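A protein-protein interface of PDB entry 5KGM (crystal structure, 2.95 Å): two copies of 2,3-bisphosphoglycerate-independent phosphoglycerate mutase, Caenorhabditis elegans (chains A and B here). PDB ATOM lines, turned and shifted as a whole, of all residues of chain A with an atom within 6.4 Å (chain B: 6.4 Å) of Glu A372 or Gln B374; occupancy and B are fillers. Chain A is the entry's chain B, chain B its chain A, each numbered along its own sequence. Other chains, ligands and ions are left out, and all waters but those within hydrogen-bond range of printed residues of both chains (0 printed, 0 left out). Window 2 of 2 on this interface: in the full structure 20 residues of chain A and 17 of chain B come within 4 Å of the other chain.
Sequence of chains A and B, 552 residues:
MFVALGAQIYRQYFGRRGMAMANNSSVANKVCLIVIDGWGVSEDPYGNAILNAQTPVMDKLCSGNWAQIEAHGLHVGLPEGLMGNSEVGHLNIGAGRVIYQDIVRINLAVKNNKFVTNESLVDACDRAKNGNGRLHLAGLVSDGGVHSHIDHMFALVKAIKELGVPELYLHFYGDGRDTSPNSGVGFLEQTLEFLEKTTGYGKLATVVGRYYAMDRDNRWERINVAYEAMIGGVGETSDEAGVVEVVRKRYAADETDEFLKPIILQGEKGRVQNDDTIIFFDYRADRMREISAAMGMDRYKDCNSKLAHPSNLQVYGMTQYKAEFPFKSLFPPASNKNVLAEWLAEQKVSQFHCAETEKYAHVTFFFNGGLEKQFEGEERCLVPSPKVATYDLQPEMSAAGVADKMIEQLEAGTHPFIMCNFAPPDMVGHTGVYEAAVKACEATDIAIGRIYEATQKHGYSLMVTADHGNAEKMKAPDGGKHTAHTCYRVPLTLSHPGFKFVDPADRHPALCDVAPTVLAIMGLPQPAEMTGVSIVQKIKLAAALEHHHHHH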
ATOM      1  N   PHE A 365     -14.693  18.010  -5.221  1.00  0.00           N
ATOM      2  CA  PHE A 365     -15.086  16.611  -5.362  1.00  0.00           C
ATOM      3  C   PHE A 365     -15.586  16.034  -4.036  1.00  0.00           C
ATOM      4  O   PHE A 365     -16.704  15.517  -3.953  1.00  0.00           O
ATOM      5  CB  PHE A 365     -13.890  15.822  -5.888  1.00  0.00           C
ATOM      6  CG  PHE A 365     -14.146  14.372  -6.072  1.00  0.00           C
ATOM      7  CD1 PHE A 365     -14.542  13.879  -7.303  1.00  0.00           C
ATOM      8  CD2 PHE A 365     -13.933  13.489  -5.036  1.00  0.00           C
ATOM      9  CE1 PHE A 365     -14.761  12.544  -7.477  1.00  0.00           C
ATOM     10  CE2 PHE A 365     -14.152  12.144  -5.206  1.00  0.00           C
ATOM     11  CZ  PHE A 365     -14.562  11.670  -6.420  1.00  0.00           C
ATOM     12  N   GLY A 370     -18.280  13.311  -2.665  1.00  0.00           N
ATOM     13  CA  GLY A 370     -17.430  12.278  -3.236  1.00  0.00           C
ATOM     14  C   GLY A 370     -17.729  11.951  -4.689  1.00  0.00           C
ATOM     15  O   GLY A 370     -17.691  10.776  -5.074  1.00  0.00           O
ATOM     16  N   LEU A 371     -18.010  12.960  -5.513  1.00  0.00           N
ATOM     17  CA  LEU A 371     -18.254  12.755  -6.939  1.00  0.00           C
ATOM     18  C   LEU A 371     -17.960  14.032  -7.720  1.00  0.00           C
ATOM     19  O   LEU A 371     -17.978  15.143  -7.181  1.00  0.00           O
ATOM     20  CB  LEU A 371     -19.698  12.326  -7.220  1.00  0.00           C
ATOM     21  CG  LEU A 371     -20.751  13.444  -7.227  1.00  0.00           C
ATOM     22  CD1 LEU A 371     -22.099  12.886  -7.564  1.00  0.00           C
ATOM     23  CD2 LEU A 371     -20.820  14.115  -5.869  1.00  0.00           C
ATOM     24  N   GLU A 372     -17.710  13.853  -9.015  1.00  0.00           N
ATOM     25  CA  GLU A 372     -17.454  14.978  -9.912  1.00  0.00           C
ATOM     26  C   GLU A 372     -18.796  15.582 -10.297  1.00  0.00           C
ATOM     27  O   GLU A 372     -19.456  15.111 -11.225  1.00  0.00           O
ATOM     28  CB  GLU A 372     -16.685  14.495 -11.139  1.00  0.00           C
ATOM     29  CG  GLU A 372     -16.296  15.562 -12.125  1.00  0.00           C
ATOM     30  CD  GLU A 372     -15.215  16.454 -11.573  1.00  0.00           C
ATOM     31  OE1 GLU A 372     -14.245  15.886 -11.018  1.00  0.00           O
ATOM     32  OE2 GLU A 372     -15.346  17.704 -11.670  1.00  0.00           O
ATOM     33  N   LYS A 373     -19.199  16.639  -9.584  1.00  0.00           N
ATOM     34  CA  LYS A 373     -20.447  17.325  -9.896  1.00  0.00           C
ATOM     35  C   LYS A 373     -20.477  18.782  -9.452  1.00  0.00           C
ATOM     36  O   LYS A 373     -20.170  19.076  -8.292  1.00  0.00           O
ATOM     37  CB  LYS A 373     -21.606  16.572  -9.243  1.00  0.00           C
ATOM     38  CG  LYS A 373     -23.002  17.122  -9.491  1.00  0.00           C
ATOM     39  CD  LYS A 373     -23.351  17.229 -10.944  1.00  0.00           C
ATOM     40  CE  LYS A 373     -24.683  17.938 -11.128  1.00  0.00           C
ATOM     41  NZ  LYS A 373     -25.790  16.972 -10.797  1.00  0.00           N
ATOM     42  N   GLN A 374     -20.764  19.696 -10.369  1.00  0.00           N
ATOM     43  CA  GLN A 374     -20.916  21.098 -10.003  1.00  0.00           C
ATOM     44  C   GLN A 374     -22.399  21.433 -10.157  1.00  0.00           C
ATOM     45  O   GLN A 374     -22.989  21.192 -11.215  1.00  0.00           O
ATOM     46  CB  GLN A 374     -20.031  22.007 -10.863  1.00  0.00           C
ATOM     47  CG  GLN A 374     -20.015  23.465 -10.419  1.00  0.00           C
ATOM     48  CD  GLN A 374     -18.993  24.323 -11.168  1.00  0.00           C
ATOM     49  OE1 GLN A 374     -18.121  23.813 -11.877  1.00  0.00           O
ATOM     50  NE2 GLN A 374     -19.079  25.632 -10.978  1.00  0.00           N
ATOM     51  N   ARG A 380     -16.924  28.131  -8.382  1.00  0.00           N
ATOM     52  CA  ARG A 380     -15.708  27.606  -7.787  1.00  0.00           C
ATOM     53  C   ARG A 380     -14.538  28.515  -8.130  1.00  0.00           C
ATOM     54  O   ARG A 380     -14.574  29.230  -9.138  1.00  0.00           O
ATOM     55  CB  ARG A 380     -15.421  26.196  -8.266  1.00  0.00           C
ATOM     56  CG  ARG A 380     -16.399  25.196  -7.752  1.00  0.00           C
ATOM     57  CD  ARG A 380     -16.276  23.880  -8.489  1.00  0.00           C
ATOM     58  NE  ARG A 380     -17.156  22.861  -7.921  1.00  0.00           N
ATOM     59  CZ  ARG A 380     -17.137  21.579  -8.261  1.00  0.00           C
ATOM     60  NH1 ARG A 380     -16.280  21.142  -9.186  1.00  0.00           N
ATOM     61  NH2 ARG A 380     -17.980  20.737  -7.667  1.00  0.00           N
ATOM     62  N   TYR B 360      -5.166  15.040  -8.901  1.00  0.00           N
ATOM     63  CA  TYR B 360      -6.448  15.020  -9.586  1.00  0.00           C
ATOM     64  C   TYR B 360      -6.738  16.360 -10.252  1.00  0.00           C
ATOM     65  O   TYR B 360      -7.053  16.408 -11.451  1.00  0.00           O
ATOM     66  CB  TYR B 360      -7.553  14.615  -8.606  1.00  0.00           C
ATOM     67  CG  TYR B 360      -8.898  14.498  -9.275  1.00  0.00           C
ATOM     68  CD1 TYR B 360      -9.179  13.385 -10.047  1.00  0.00           C
ATOM     69  CD2 TYR B 360      -9.876  15.469  -9.146  1.00  0.00           C
ATOM     70  CE1 TYR B 360     -10.386  13.241 -10.685  1.00  0.00           C
ATOM     71  CE2 TYR B 360     -11.100  15.335  -9.788  1.00  0.00           C
ATOM     72  CZ  TYR B 360     -11.349  14.213 -10.553  1.00  0.00           C
ATOM     73  OH  TYR B 360     -12.555  14.039 -11.204  1.00  0.00           O
ATOM     74  N   THR B 364      -7.436  17.442 -14.445  1.00  0.00           N
ATOM     75  CA  THR B 364      -8.740  18.046 -14.716  1.00  0.00           C
ATOM     76  C   THR B 364      -8.646  19.548 -14.971  1.00  0.00           C
ATOM     77  O   THR B 364      -8.551  19.976 -16.125  1.00  0.00           O
ATOM     78  CB  THR B 364      -9.696  17.770 -13.549  1.00  0.00           C
ATOM     79  OG1 THR B 364      -9.090  18.162 -12.308  1.00  0.00           O
ATOM     80  CG2 THR B 364     -10.033  16.300 -13.475  1.00  0.00           C
ATOM     81  N   ASN B 368      -7.232  20.699 -18.722  1.00  0.00           N
ATOM     82  CA  ASN B 368      -8.247  21.257 -19.608  1.00  0.00           C
ATOM     83  C   ASN B 368      -8.078  22.762 -19.878  1.00  0.00           C
ATOM     84  O   ASN B 368      -8.985  23.376 -20.459  1.00  0.00           O
ATOM     85  CB  ASN B 368      -9.635  20.998 -19.031  1.00  0.00           C
ATOM     86  CG  ASN B 368     -10.107  19.591 -19.274  1.00  0.00           C
ATOM     87  OD1 ASN B 368      -9.329  18.717 -19.636  1.00  0.00           O
ATOM     88  ND2 ASN B 368     -11.387  19.352 -19.035  1.00  0.00           N
ATOM     89  N   LEU B 371      -9.324  25.839 -16.096  1.00  0.00           N
ATOM     90  CA  LEU B 371     -10.674  26.279 -15.744  1.00  0.00           C
ATOM     91  C   LEU B 371     -11.515  25.086 -15.305  1.00  0.00           C
ATOM     92  O   LEU B 371     -11.172  23.927 -15.573  1.00  0.00           O
ATOM     93  CB  LEU B 371     -11.405  26.922 -16.935  1.00  0.00           C
ATOM     94  CG  LEU B 371     -11.987  25.908 -17.936  1.00  0.00           C
ATOM     95  CD1 LEU B 371     -12.757  26.608 -19.054  1.00  0.00           C
ATOM     96  CD2 LEU B 371     -10.940  24.957 -18.491  1.00  0.00           C
ATOM     97  N   GLU B 372     -12.657  25.389 -14.658  1.00  0.00           N
ATOM     98  CA  GLU B 372     -13.583  24.351 -14.200  1.00  0.00           C
ATOM     99  C   GLU B 372     -14.651  24.141 -15.267  1.00  0.00           C
ATOM    100  O   GLU B 372     -15.673  24.829 -15.311  1.00  0.00           O
ATOM    101  CB  GLU B 372     -14.189  24.736 -12.852  1.00  0.00           C
ATOM    102  CG  GLU B 372     -14.780  23.580 -12.000  1.00  0.00           C
ATOM    103  CD  GLU B 372     -13.759  22.593 -11.501  1.00  0.00           C
ATOM    104  OE1 GLU B 372     -12.996  22.916 -10.575  1.00  0.00           O
ATOM    105  OE2 GLU B 372     -13.770  21.450 -11.998  1.00  0.00           O
ATOM    106  N   LYS B 373     -14.405  23.155 -16.127  1.00  0.00           N
ATOM    107  CA  LYS B 373     -15.299  22.798 -17.221  1.00  0.00           C
ATOM    108  C   LYS B 373     -15.040  21.348 -17.577  1.00  0.00           C
ATOM    109  O   LYS B 373     -13.881  20.942 -17.721  1.00  0.00           O
ATOM    110  CB  LYS B 373     -15.185  23.674 -18.482  1.00  0.00           C
ATOM    111  CG  LYS B 373     -16.265  23.259 -19.532  1.00  0.00           C
ATOM    112  CD  LYS B 373     -16.900  24.406 -20.319  1.00  0.00           C
ATOM    113  CE  LYS B 373     -15.920  25.091 -21.263  1.00  0.00           C
ATOM    114  NZ  LYS B 373     -16.602  25.805 -22.398  1.00  0.00           N
ATOM    115  N   GLN B 374     -16.099  20.573 -17.687  1.00  0.00           N
ATOM    116  CA  GLN B 374     -15.984  19.189 -18.102  1.00  0.00           C
ATOM    117  C   GLN B 374     -16.693  19.092 -19.443  1.00  0.00           C
ATOM    118  O   GLN B 374     -17.899  19.346 -19.535  1.00  0.00           O
ATOM    119  CB  GLN B 374     -16.613  18.248 -17.076  1.00  0.00           C
ATOM    120  CG  GLN B 374     -16.517  16.779 -17.419  1.00  0.00           C
ATOM    121  CD  GLN B 374     -16.924  15.902 -16.263  1.00  0.00           C
ATOM    122  OE1 GLN B 374     -17.312  16.397 -15.210  1.00  0.00           O
ATOM    123  NE2 GLN B 374     -16.854  14.593 -16.454  1.00  0.00           N
ATOM    124  N   PHE B 375     -15.974  18.632 -20.452  1.00  0.00           N
ATOM    125  CA  PHE B 375     -16.521  18.681 -21.792  1.00  0.00           C
ATOM    126  C   PHE B 375     -17.353  17.436 -22.055  1.00  0.00           C
ATOM    127  O   PHE B 375     -17.199  16.393 -21.407  1.00  0.00           O
ATOM    128  CB  PHE B 375     -15.398  18.832 -22.812  1.00  0.00           C
ATOM    129  CG  PHE B 375     -14.640  20.133 -22.683  1.00  0.00           C
ATOM    130  CD1 PHE B 375     -15.154  21.299 -23.218  1.00  0.00           C
ATOM    131  CD2 PHE B 375     -13.452  20.204 -21.962  1.00  0.00           C
ATOM    132  CE1 PHE B 375     -14.470  22.480 -23.092  1.00  0.00           C
ATOM    133  CE2 PHE B 375     -12.767  21.408 -21.822  1.00  0.00           C
ATOM    134  CZ  PHE B 375     -13.280  22.535 -22.374  1.00  0.00           C
ATOM    135  N   GLU B 376     -18.256  17.573 -23.015  1.00  0.00           N
ATOM    136  CA  GLU B 376     -19.110  16.466 -23.392  1.00  0.00           C
ATOM    137  C   GLU B 376     -18.270  15.271 -23.819  1.00  0.00           C
ATOM    138  O   GLU B 376     -17.306  15.396 -24.586  1.00  0.00           O
ATOM    139  CB  GLU B 376     -20.054  16.905 -24.506  1.00  0.00           C
ATOM    140  CG  GLU B 376     -21.092  15.869 -24.872  1.00  0.00           C
ATOM    141  CD  GLU B 376     -22.078  16.370 -25.908  1.00  0.00           C
ATOM    142  OE1 GLU B 376     -21.937  17.539 -26.340  1.00  0.00           O
ATOM    143  OE2 GLU B 376     -22.977  15.586 -26.299  1.00  0.00           O
ATOM    144  N   GLU B 378     -16.390  13.541 -21.782  1.00  0.00           N
ATOM    145  CA  GLU B 378     -15.241  13.358 -20.902  1.00  0.00           C
ATOM    146  C   GLU B 378     -15.669  12.637 -19.622  1.00  0.00           C
ATOM    147  O   GLU B 378     -16.547  13.115 -18.896  1.00  0.00           O
ATOM    148  CB  GLU B 378     -14.604  14.707 -20.562  1.00  0.00           C
ATOM    149  CG  GLU B 378     -13.447  14.613 -19.561  1.00  0.00           C
ATOM    150  CD  GLU B 378     -12.906  15.965 -19.106  1.00  0.00           C
ATOM    151  OE1 GLU B 378     -13.227  16.990 -19.743  1.00  0.00           O
ATOM    152  OE2 GLU B 378     -12.099  15.986 -18.152  1.00  0.00           O
ATOM    153  N   GLU B 379     -15.058  11.483 -19.352  1.00  0.00           N
ATOM    154  CA  GLU B 379     -15.289  10.751 -18.118  1.00  0.00           C
ATOM    155  C   GLU B 379     -14.059  10.909 -17.237  1.00  0.00           C
ATOM    156  O   GLU B 379     -12.928  10.780 -17.717  1.00  0.00           O
ATOM    157  CB  GLU B 379     -15.554   9.272 -18.418  1.00  0.00           C
ATOM    158  CG  GLU B 379     -15.790   8.391 -17.204  1.00  0.00           C
ATOM    159  CD  GLU B 379     -16.192   6.973 -17.582  1.00  0.00           C
ATOM    160  OE1 GLU B 379     -16.413   6.720 -18.782  1.00  0.00           O
ATOM    161  OE2 GLU B 379     -16.282   6.109 -16.683  1.00  0.00           O
ATOM    162  N   ARG B 380     -14.279  11.140 -15.943  1.00  0.00           N
ATOM    163  CA  ARG B 380     -13.204  11.402 -14.995  1.00  0.00           C
ATOM    164  C   ARG B 380     -13.211  10.357 -13.892  1.00  0.00           C
ATOM    165  O   ARG B 380     -14.241   9.737 -13.627  1.00  0.00           O
ATOM    166  CB  ARG B 380     -13.298  12.796 -14.380  1.00  0.00           C
ATOM    167  CG  ARG B 380     -12.963  13.892 -15.352  1.00  0.00           C
ATOM    168  CD  ARG B 380     -13.339  15.265 -14.787  1.00  0.00           C
ATOM    169  NE  ARG B 380     -12.905  16.361 -15.648  1.00  0.00           N
ATOM    170  CZ  ARG B 380     -12.931  17.643 -15.304  1.00  0.00           C
ATOM    171  NH1 ARG B 380     -13.379  18.002 -14.102  1.00  0.00           N
ATOM    172  NH2 ARG B 380     -12.510  18.565 -16.167  1.00  0.00           N
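O of Tyr B360 sits at hydrogen-bond distance from OG1 of Thr B364, at 2.8 Å.
The side-chain amide nitrogen (ND2) of Asn B368 sits close to the guanidinium group (NH2) of Arg B380 (3.2 Å).
The backbone carbonyl oxygen (O) of Lys B373 sits at hydrogen-bond distance from the guanidinium group (NH2) of Arg B380, at 3.2 Å.
NE2 of Gln B374 is in hydrogen-bond range of O of Glu B378 (2.9 Å).
OE2 of Glu B378 lies within salt-bridge range of NE of Arg B380, at 2.7 Å.
NH2 of Arg A380 sits at hydrogen-bond distance from O of Lys A373 (2.8 Å).
Of the 12 printed residues of chain B, 4 touch a printed residue of chain A.
Printed residues of chain B that touch a printed residue of chain A: Tyr B360, Glu B372, Gln B374 and Arg B380.
Among the printed residues, 5 pairs touch across the chains.
Glu A372 touches Gln B374, and with the chains exchanged Gln A374 touches Glu B372.
Glu A372 touches Arg B380, and with the chains exchanged Arg A380 touches Glu B372.
Of the 5 pairs that touch across the chains among the printed residues, 4 have their exchanged pair printed and touching as well.
Among the printed residues, pairs that only touch across the chains: Glu A372 with Gln B374 and Gln A374 with Glu B372.
The side-chain hydroxyl (OH) of Tyr B360 sits at hydrogen-bond distance from the side-chain carboxylate (OE1) of Glu A372 (2.5 Å).
The side-chain carboxylate (OE2) of Glu B372 is in salt-bridge range of the guanidinium group (NH1) of Arg A380 (3.8 Å).
The guanidinium group (NH1) of Arg B380 lies within salt-bridge range of the side-chain carboxylate (OE2) of Glu A372, 3.1 Å away.
Of the printed residues of chain B, Glu A372 touches Tyr B360 (2.5 Å), Gln B374 (3.4 Å) and Arg B380 (3.1 Å).
Printed residues of chain B within 4 Å of Gln A374: Glu B372.
Of the printed residues of chain B, Arg A380 touches Glu B372 (3.7 Å).
Thr B364 touches none of the printed residues of chain A.
Gln B374 touches one residue of chain A.
The nearest printed residue of chain A that does not touch Arg B380 is Arg A380 (6.5 Å).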
